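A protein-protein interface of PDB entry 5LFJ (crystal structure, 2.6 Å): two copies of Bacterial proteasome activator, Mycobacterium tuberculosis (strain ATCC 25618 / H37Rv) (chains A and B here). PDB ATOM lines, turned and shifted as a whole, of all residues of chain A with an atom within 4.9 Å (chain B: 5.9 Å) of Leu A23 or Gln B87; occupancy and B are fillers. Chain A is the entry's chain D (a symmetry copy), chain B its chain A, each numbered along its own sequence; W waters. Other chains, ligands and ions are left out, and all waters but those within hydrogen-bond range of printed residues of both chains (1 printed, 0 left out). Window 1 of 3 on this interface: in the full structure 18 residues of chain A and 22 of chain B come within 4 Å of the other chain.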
ATOM      1  N   MET A  19     -14.241 -16.458  21.350  1.00  0.00           N
ATOM      2  CA  MET A  19     -15.220 -16.668  22.414  1.00  0.00           C
ATOM      3  C   MET A  19     -16.604 -16.188  21.980  1.00  0.00           C
ATOM      4  O   MET A  19     -17.618 -16.892  22.152  1.00  0.00           O
ATOM      5  CB  MET A  19     -14.787 -15.920  23.666  1.00  0.00           C
ATOM      6  CG  MET A  19     -15.739 -16.103  24.810  1.00  0.00           C
ATOM      7  SD  MET A  19     -15.327 -15.066  26.210  1.00  0.00           S
ATOM      8  CE  MET A  19     -15.927 -13.483  25.615  1.00  0.00           C
ATOM      9  N   ILE A  20     -16.667 -14.969  21.435  1.00  0.00           N
ATOM     10  CA  ILE A  20     -17.947 -14.401  21.025  1.00  0.00           C
ATOM     11  C   ILE A  20     -18.552 -15.202  19.879  1.00  0.00           C
ATOM     12  O   ILE A  20     -19.766 -15.440  19.851  1.00  0.00           O
ATOM     13  CB  ILE A  20     -17.775 -12.918  20.661  1.00  0.00           C
ATOM     14  CG1 ILE A  20     -17.419 -12.112  21.907  1.00  0.00           C
ATOM     15  CG2 ILE A  20     -19.027 -12.375  20.004  1.00  0.00           C
ATOM     16  CD1 ILE A  20     -17.004 -10.677  21.596  1.00  0.00           C
ATOM     17  N   LYS A  21     -17.731 -15.606  18.903  1.00  0.00           N
ATOM     18  CA  LYS A  21     -18.249 -16.388  17.779  1.00  0.00           C
ATOM     19  C   LYS A  21     -18.836 -17.706  18.262  1.00  0.00           C
ATOM     20  O   LYS A  21     -19.905 -18.133  17.802  1.00  0.00           O
ATOM     21  CB  LYS A  21     -17.149 -16.601  16.726  1.00  0.00           C
ATOM     22  CG  LYS A  21     -17.626 -17.275  15.430  1.00  0.00           C
ATOM     23  CD  LYS A  21     -16.550 -17.309  14.315  1.00  0.00           C
ATOM     24  CE  LYS A  21     -15.489 -18.393  14.532  1.00  0.00           C
ATOM     25  NZ  LYS A  21     -14.483 -18.456  13.425  1.00  0.00           N
ATOM     26  N   GLN A  22     -18.150 -18.366  19.201  1.00  0.00           N
ATOM     27  CA  GLN A  22     -18.654 -19.621  19.754  1.00  0.00           C
ATOM     28  C   GLN A  22     -19.996 -19.412  20.470  1.00  0.00           C
ATOM     29  O   GLN A  22     -20.922 -20.229  20.340  1.00  0.00           O
ATOM     30  CB  GLN A  22     -17.611 -20.179  20.725  1.00  0.00           C
ATOM     31  CG  GLN A  22     -17.766 -21.621  21.155  1.00  0.00           C
ATOM     32  CD  GLN A  22     -17.317 -22.586  20.076  1.00  0.00           C
ATOM     33  OE1 GLN A  22     -16.164 -22.523  19.613  1.00  0.00           O
ATOM     34  NE2 GLN A  22     -18.205 -23.501  19.683  1.00  0.00           N
ATOM     35  N   LEU A  23     -20.126 -18.303  21.220  1.00  0.00           N
ATOM     36  CA  LEU A  23     -21.389 -18.018  21.906  1.00  0.00           C
ATOM     37  C   LEU A  23     -22.516 -17.719  20.921  1.00  0.00           C
ATOM     38  O   LEU A  23     -23.661 -18.139  21.132  1.00  0.00           O
ATOM     39  CB  LEU A  23     -21.223 -16.858  22.889  1.00  0.00           C
ATOM     40  CG  LEU A  23     -20.389 -17.071  24.155  1.00  0.00           C
ATOM     41  CD1 LEU A  23     -20.174 -15.770  24.918  1.00  0.00           C
ATOM     42  CD2 LEU A  23     -21.048 -18.092  25.054  1.00  0.00           C
ATOM     43  N   LEU A  24     -22.233 -16.943  19.876  1.00  0.00           N
ATOM     44  CA  LEU A  24     -23.225 -16.730  18.826  1.00  0.00           C
ATOM     45  C   LEU A  24     -23.698 -18.055  18.243  1.00  0.00           C
ATOM     46  O   LEU A  24     -24.900 -18.252  18.009  1.00  0.00           O
ATOM     47  CB  LEU A  24     -22.656 -15.814  17.737  1.00  0.00           C
ATOM     48  CG  LEU A  24     -23.564 -15.609  16.527  1.00  0.00           C
ATOM     49  CD1 LEU A  24     -24.852 -14.919  16.953  1.00  0.00           C
ATOM     50  CD2 LEU A  24     -22.855 -14.808  15.464  1.00  0.00           C
ATOM     51  N   GLU A  25     -22.767 -18.976  17.989  1.00  0.00           N
ATOM     52  CA  GLU A  25     -23.176 -20.280  17.474  1.00  0.00           C
ATOM     53  C   GLU A  25     -24.080 -20.999  18.468  1.00  0.00           C
ATOM     54  O   GLU A  25     -25.053 -21.661  18.069  1.00  0.00           O
ATOM     55  CB  GLU A  25     -21.943 -21.108  17.113  1.00  0.00           C
ATOM     56  CG  GLU A  25     -21.185 -20.490  15.928  1.00  0.00           C
ATOM     57  CD  GLU A  25     -19.864 -21.177  15.588  1.00  0.00           C
ATOM     58  OE1 GLU A  25     -19.436 -22.085  16.333  1.00  0.00           O
ATOM     59  OE2 GLU A  25     -19.229 -20.771  14.587  1.00  0.00           O
ATOM     60  N   GLU A  26     -23.819 -20.835  19.772  1.00  0.00           N
ATOM     61  CA  GLU A  26     -24.707 -21.463  20.757  1.00  0.00           C
ATOM     62  C   GLU A  26     -26.101 -20.849  20.758  1.00  0.00           C
ATOM     63  O   GLU A  26     -27.090 -21.578  20.883  1.00  0.00           O
ATOM     64  CB  GLU A  26     -24.119 -21.393  22.165  1.00  0.00           C
ATOM     65  CG  GLU A  26     -23.069 -22.427  22.408  1.00  0.00           C
ATOM     66  CD  GLU A  26     -23.574 -23.836  22.218  1.00  0.00           C
ATOM     67  OE1 GLU A  26     -24.722 -24.114  22.611  1.00  0.00           O
ATOM     68  OE2 GLU A  26     -22.820 -24.664  21.665  1.00  0.00           O
ATOM     69  N   VAL A  27     -26.212 -19.520  20.666  1.00  0.00           N
ATOM     70  CA  VAL A  27     -27.545 -18.912  20.684  1.00  0.00           C
ATOM     71  C   VAL A  27     -28.330 -19.341  19.453  1.00  0.00           C
ATOM     72  O   VAL A  27     -29.531 -19.630  19.535  1.00  0.00           O
ATOM     73  CB  VAL A  27     -27.466 -17.378  20.822  1.00  0.00           C
ATOM     74  CG1 VAL A  27     -26.645 -17.022  22.008  1.00  0.00           C
ATOM     75  CG2 VAL A  27     -26.904 -16.718  19.602  1.00  0.00           C
ATOM     76  N   ARG A  39     -26.982 -13.651  31.723  1.00  0.00           N
ATOM     77  CA  ARG A  39     -25.558 -13.958  31.720  1.00  0.00           C
ATOM     78  C   ARG A  39     -24.912 -13.545  30.410  1.00  0.00           C
ATOM     79  O   ARG A  39     -23.838 -12.932  30.397  1.00  0.00           O
ATOM     80  CB  ARG A  39     -25.342 -15.458  31.960  1.00  0.00           C
ATOM     81  CG  ARG A  39     -23.883 -15.920  31.716  1.00  0.00           C
ATOM     82  CD  ARG A  39     -23.655 -17.458  31.786  1.00  0.00           C
ATOM     83  NE  ARG A  39     -23.541 -18.014  33.131  1.00  0.00           N
ATOM     84  CZ  ARG A  39     -22.411 -18.023  33.838  1.00  0.00           C
ATOM     85  NH1 ARG A  39     -21.301 -17.495  33.324  1.00  0.00           N
ATOM     86  NH2 ARG A  39     -22.386 -18.560  35.057  1.00  0.00           N
ATOM     87  N   LEU A  40     -25.574 -13.855  29.296  1.00  0.00           N
ATOM     88  CA  LEU A  40     -25.002 -13.570  27.988  1.00  0.00           C
ATOM     89  C   LEU A  40     -24.909 -12.067  27.748  1.00  0.00           C
ATOM     90  O   LEU A  40     -23.947 -11.587  27.130  1.00  0.00           O
ATOM     91  CB  LEU A  40     -25.833 -14.272  26.927  1.00  0.00           C
ATOM     92  CG  LEU A  40     -25.282 -14.273  25.519  1.00  0.00           C
ATOM     93  CD1 LEU A  40     -23.909 -14.911  25.511  1.00  0.00           C
ATOM     94  CD2 LEU A  40     -26.248 -15.105  24.744  1.00  0.00           C
ATOM     95  N   ILE A  43     -21.782 -11.032  29.620  1.00  0.00           N
ATOM     96  CA  ILE A  43     -20.615 -11.418  28.841  1.00  0.00           C
ATOM     97  C   ILE A  43     -20.373 -10.430  27.707  1.00  0.00           C
ATOM     98  O   ILE A  43     -19.231 -10.039  27.443  1.00  0.00           O
ATOM     99  CB  ILE A  43     -20.793 -12.843  28.301  1.00  0.00           C
ATOM    100  CG1 ILE A  43     -20.786 -13.839  29.450  1.00  0.00           C
ATOM    101  CG2 ILE A  43     -19.666 -13.171  27.302  1.00  0.00           C
ATOM    102  CD1 ILE A  43     -21.130 -15.230  29.007  1.00  0.00           C
ATOM    103  N   GLN A  85     -24.088  -9.653  19.070  1.00  0.00           N
ATOM    104  CA  GLN A  85     -22.902 -10.478  18.883  1.00  0.00           C
ATOM    105  C   GLN A  85     -22.532 -10.654  17.415  1.00  0.00           C
ATOM    106  O   GLN A  85     -21.348 -10.715  17.080  1.00  0.00           O
ATOM    107  CB  GLN A  85     -23.083 -11.829  19.560  1.00  0.00           C
ATOM    108  CG  GLN A  85     -23.069 -11.731  21.069  1.00  0.00           C
ATOM    109  CD  GLN A  85     -23.037 -13.077  21.732  1.00  0.00           C
ATOM    110  OE1 GLN A  85     -23.419 -14.080  21.133  1.00  0.00           O
ATOM    111  NE2 GLN A  85     -22.459 -13.132  22.927  1.00  0.00           N
ATOM    112  N   LEU B  66     -14.039 -12.478  32.804  1.00  0.00           N
ATOM    113  CA  LEU B  66     -14.979 -12.886  31.765  1.00  0.00           C
ATOM    114  C   LEU B  66     -16.038 -13.864  32.250  1.00  0.00           C
ATOM    115  O   LEU B  66     -17.088 -13.979  31.611  1.00  0.00           O
ATOM    116  CB  LEU B  66     -14.223 -13.529  30.595  1.00  0.00           C
ATOM    117  CG  LEU B  66     -13.301 -12.634  29.761  1.00  0.00           C
ATOM    118  CD1 LEU B  66     -12.410 -13.458  28.837  1.00  0.00           C
ATOM    119  CD2 LEU B  66     -14.135 -11.663  28.943  1.00  0.00           C
ATOM    120  N   THR B  67     -15.796 -14.561  33.355  1.00  0.00           N
ATOM    121  CA  THR B  67     -16.681 -15.609  33.837  1.00  0.00           C
ATOM    122  C   THR B  67     -17.298 -15.216  35.166  1.00  0.00           C
ATOM    123  O   THR B  67     -16.620 -14.682  36.051  1.00  0.00           O
ATOM    124  CB  THR B  67     -15.945 -16.922  34.022  1.00  0.00           C
ATOM    125  OG1 THR B  67     -14.932 -16.757  35.023  1.00  0.00           O
ATOM    126  CG2 THR B  67     -15.299 -17.328  32.727  1.00  0.00           C
ATOM    127  N   LEU B  68     -18.577 -15.501  35.299  1.00  0.00           N
ATOM    128  CA  LEU B  68     -19.240 -15.366  36.574  1.00  0.00           C
ATOM    129  C   LEU B  68     -19.568 -16.778  37.033  1.00  0.00           C
ATOM    130  O   LEU B  68     -20.056 -17.576  36.221  1.00  0.00           O
ATOM    131  CB  LEU B  68     -20.521 -14.525  36.420  1.00  0.00           C
ATOM    132  CG  LEU B  68     -21.238 -13.797  37.569  1.00  0.00           C
ATOM    133  CD1 LEU B  68     -21.636 -14.700  38.727  1.00  0.00           C
ATOM    134  CD2 LEU B  68     -20.370 -12.646  38.070  1.00  0.00           C
ATOM    135  N   ARG B  82     -24.870 -24.499  28.849  1.00  0.00           N
ATOM    136  CA  ARG B  82     -24.374 -24.479  27.485  1.00  0.00           C
ATOM    137  C   ARG B  82     -23.641 -23.163  27.202  1.00  0.00           C
ATOM    138  O   ARG B  82     -22.558 -23.159  26.592  1.00  0.00           O
ATOM    139  CB  ARG B  82     -25.572 -24.727  26.566  1.00  0.00           C
ATOM    140  CG  ARG B  82     -25.323 -25.526  25.305  1.00  0.00           C
ATOM    141  CD  ARG B  82     -26.668 -25.896  24.639  1.00  0.00           C
ATOM    142  NE  ARG B  82     -27.367 -24.732  24.101  1.00  0.00           N
ATOM    143  CZ  ARG B  82     -28.640 -24.444  24.354  1.00  0.00           C
ATOM    144  NH1 ARG B  82     -29.353 -25.242  25.136  1.00  0.00           N
ATOM    145  NH2 ARG B  82     -29.202 -23.360  23.830  1.00  0.00           N
ATOM    146  N   ILE B  83     -24.172 -22.052  27.723  1.00  0.00           N
ATOM    147  CA  ILE B  83     -23.520 -20.747  27.598  1.00  0.00           C
ATOM    148  C   ILE B  83     -22.172 -20.744  28.299  1.00  0.00           C
ATOM    149  O   ILE B  83     -21.158 -20.326  27.731  1.00  0.00           O
ATOM    150  CB  ILE B  83     -24.426 -19.632  28.152  1.00  0.00           C
ATOM    151  CG1 ILE B  83     -25.657 -19.449  27.266  1.00  0.00           C
ATOM    152  CG2 ILE B  83     -23.643 -18.343  28.365  1.00  0.00           C
ATOM    153  CD1 ILE B  83     -25.281 -19.163  25.869  1.00  0.00           C
ATOM    154  N   ALA B  84     -22.147 -21.175  29.556  1.00  0.00           N
ATOM    155  CA  ALA B  84     -20.909 -21.105  30.320  1.00  0.00           C
ATOM    156  C   ALA B  84     -19.804 -21.919  29.649  1.00  0.00           C
ATOM    157  O   ALA B  84     -18.676 -21.435  29.456  1.00  0.00           O
ATOM    158  CB  ALA B  84     -21.161 -21.597  31.746  1.00  0.00           C
ATOM    159  N   GLN B  85     -20.124 -23.163  29.271  1.00  0.00           N
ATOM    160  CA  GLN B  85     -19.104 -24.027  28.706  1.00  0.00           C
ATOM    161  C   GLN B  85     -18.704 -23.565  27.318  1.00  0.00           C
ATOM    162  O   GLN B  85     -17.531 -23.664  26.953  1.00  0.00           O
ATOM    163  CB  GLN B  85     -19.591 -25.458  28.593  1.00  0.00           C
ATOM    164  CG  GLN B  85     -20.042 -26.099  29.870  1.00  0.00           C
ATOM    165  CD  GLN B  85     -20.219 -27.582  29.699  1.00  0.00           C
ATOM    166  OE1 GLN B  85     -19.571 -28.184  28.854  1.00  0.00           O
ATOM    167  NE2 GLN B  85     -21.262 -28.115  30.290  1.00  0.00           N
ATOM    168  N   ALA B  86     -19.661 -23.072  26.532  1.00  0.00           N
ATOM    169  CA  ALA B  86     -19.325 -22.525  25.223  1.00  0.00           C
ATOM    170  C   ALA B  86     -18.381 -21.345  25.357  1.00  0.00           C
ATOM    171  O   ALA B  86     -17.435 -21.193  24.567  1.00  0.00           O
ATOM    172  CB  ALA B  86     -20.585 -22.086  24.503  1.00  0.00           C
ATOM    173  N   GLN B  87     -18.616 -20.508  26.369  1.00  0.00           N
ATOM    174  CA  GLN B  87     -17.704 -19.408  26.629  1.00  0.00           C
ATOM    175  C   GLN B  87     -16.306 -19.941  26.807  1.00  0.00           C
ATOM    176  O   GLN B  87     -15.371 -19.504  26.115  1.00  0.00           O
ATOM    177  CB  GLN B  87     -18.092 -18.659  27.893  1.00  0.00           C
ATOM    178  CG  GLN B  87     -17.379 -17.338  28.021  1.00  0.00           C
ATOM    179  CD  GLN B  87     -17.621 -16.674  29.354  1.00  0.00           C
ATOM    180  OE1 GLN B  87     -18.042 -17.320  30.329  1.00  0.00           O
ATOM    181  NE2 GLN B  87     -17.461 -15.355  29.377  1.00  0.00           N
ATOM    182  N   LEU B  88     -16.155 -20.924  27.710  1.00  0.00           N
ATOM    183  CA  LEU B  88     -14.825 -21.502  27.925  1.00  0.00           C
ATOM    184  C   LEU B  88     -14.224 -22.038  26.630  1.00  0.00           C
ATOM    185  O   LEU B  88     -13.102 -21.674  26.269  1.00  0.00           O
ATOM    186  CB  LEU B  88     -14.859 -22.589  28.993  1.00  0.00           C
ATOM    187  CG  LEU B  88     -14.900 -22.026  30.407  1.00  0.00           C
ATOM    188  CD1 LEU B  88     -14.960 -23.151  31.418  1.00  0.00           C
ATOM    189  CD2 LEU B  88     -13.684 -21.150  30.644  1.00  0.00           C
ATOM    190  N   VAL B  89     -14.976 -22.859  25.890  1.00  0.00           N
ATOM    191  CA  VAL B  89     -14.429 -23.511  24.703  1.00  0.00           C
ATOM    192  C   VAL B  89     -13.922 -22.488  23.693  1.00  0.00           C
ATOM    193  O   VAL B  89     -12.786 -22.584  23.213  1.00  0.00           O
ATOM    194  CB  VAL B  89     -15.475 -24.450  24.084  1.00  0.00           C
ATOM    195  CG1 VAL B  89     -14.995 -24.985  22.752  1.00  0.00           C
ATOM    196  CG2 VAL B  89     -15.719 -25.597  25.044  1.00  0.00           C
ATOM    197  N   GLY B  90     -14.744 -21.489  23.367  1.00  0.00           N
ATOM    198  CA  GLY B  90     -14.318 -20.490  22.403  1.00  0.00           C
ATOM    199  C   GLY B  90     -13.094 -19.735  22.879  1.00  0.00           C
ATOM    200  O   GLY B  90     -12.137 -19.531  22.121  1.00  0.00           O
ATOM    201  N   TRP B  91     -13.083 -19.360  24.156  1.00  0.00           N
ATOM    202  CA  TRP B  91     -11.948 -18.628  24.690  1.00  0.00           C
ATOM    203  C   TRP B  91     -10.664 -19.459  24.581  1.00  0.00           C
ATOM    204  O   TRP B  91      -9.598 -18.933  24.239  1.00  0.00           O
ATOM    205  CB  TRP B  91     -12.234 -18.236  26.135  1.00  0.00           C
ATOM    206  CG  TRP B  91     -11.238 -17.296  26.728  1.00  0.00           C
ATOM    207  CD1 TRP B  91     -11.231 -15.931  26.612  1.00  0.00           C
ATOM    208  CD2 TRP B  91     -10.119 -17.634  27.553  1.00  0.00           C
ATOM    209  NE1 TRP B  91     -10.167 -15.407  27.306  1.00  0.00           N
ATOM    210  CE2 TRP B  91      -9.472 -16.430  27.894  1.00  0.00           C
ATOM    211  CE3 TRP B  91      -9.595 -18.837  28.031  1.00  0.00           C
ATOM    212  CZ2 TRP B  91      -8.326 -16.398  28.682  1.00  0.00           C
ATOM    213  CZ3 TRP B  91      -8.449 -18.799  28.814  1.00  0.00           C
ATOM    214  CH2 TRP B  91      -7.831 -17.591  29.130  1.00  0.00           C
ATOM    215  N   LEU B  92     -10.761 -20.766  24.842  1.00  0.00           N
ATOM    216  CA  LEU B  92      -9.606 -21.655  24.772  1.00  0.00           C
ATOM    217  C   LEU B  92      -9.114 -21.842  23.337  1.00  0.00           C
ATOM    218  O   LEU B  92      -7.900 -21.791  23.070  1.00  0.00           O
ATOM    219  CB  LEU B  92      -9.972 -22.996  25.397  1.00  0.00           C
ATOM    220  CG  LEU B  92     -10.237 -22.979  26.904  1.00  0.00           C
ATOM    221  CD1 LEU B  92     -10.786 -24.328  27.369  1.00  0.00           C
ATOM    222  CD2 LEU B  92      -8.941 -22.662  27.641  1.00  0.00           C
HETATM  223  O   HOH W   1     -18.482 -19.025  34.401  1.00  0.00           O
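Water W1 bridges O of Leu B68 (2.8 Å) and NH1 of Arg A39 (3.4 Å).
The guanidinium group (NH2) of Arg A39 sits at hydrogen-bond distance from the backbone carbonyl oxygen (O) of Leu B68. OE1 of Glu A26 is in salt-bridge range of NE of Arg B82 (3.1 Å).
1 position is printed for both chains. Of the 12 pairs that touch across the chains among the printed residues, none has its exchanged pair printed and touching as well.
The backbone carbonyl oxygen (O) of Leu B66 lies within hydrogen-bond range of the side-chain amide nitrogen (NE2) of Gln B87 (2.7 Å).
Of the 13 printed residues of chain A, 6 touch a printed residue of chain B. Printed residues of chain A that touch a printed residue of chain B: Met A19, Gln A22, Leu A23, Glu A26, Arg A39 and Ile A43. Hydrophobic or aromatic side chains of chain A that line the printed part of chain B: Met A19, Leu A23 and Ile A43. Along chain B the printed residues that touch a printed residue of chain A span positions 68 to 91.
Of chain B, only Ile B83 (3.5 Å) and Gln B87 (3.7 Å) come within 4 Å of Leu A23. Of the printed residues of chain B, Ile A43 touches Gln B87. Printed residues of chain A within 4 Å of Arg B82: Glu A26. Gln B85 touches none of the printed residues of chain A. Gln B87 touches three residues of chain A. Of the printed residues of chain A, Gly B90 touches Met A19 and Gln A22. Leu B92 touches none of the printed residues of chain A. The nearest printed residue of chain A that does not touch Ile B83 is Ile A43 (4.1 Å).
Among the printed residues, pairs that only touch across the chains: Glu A26 with Ala B86, Gln A22 with Ala B86, Leu A23 with Ile B83, Arg A39 with Ile B83, Met A19 with Gln B87, Ile A43 with Gln B87, Leu A23 with Gln B87, Gln A22 with Gly B90, Met A19 with Gly B90 and Met A19 with Trp B91.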
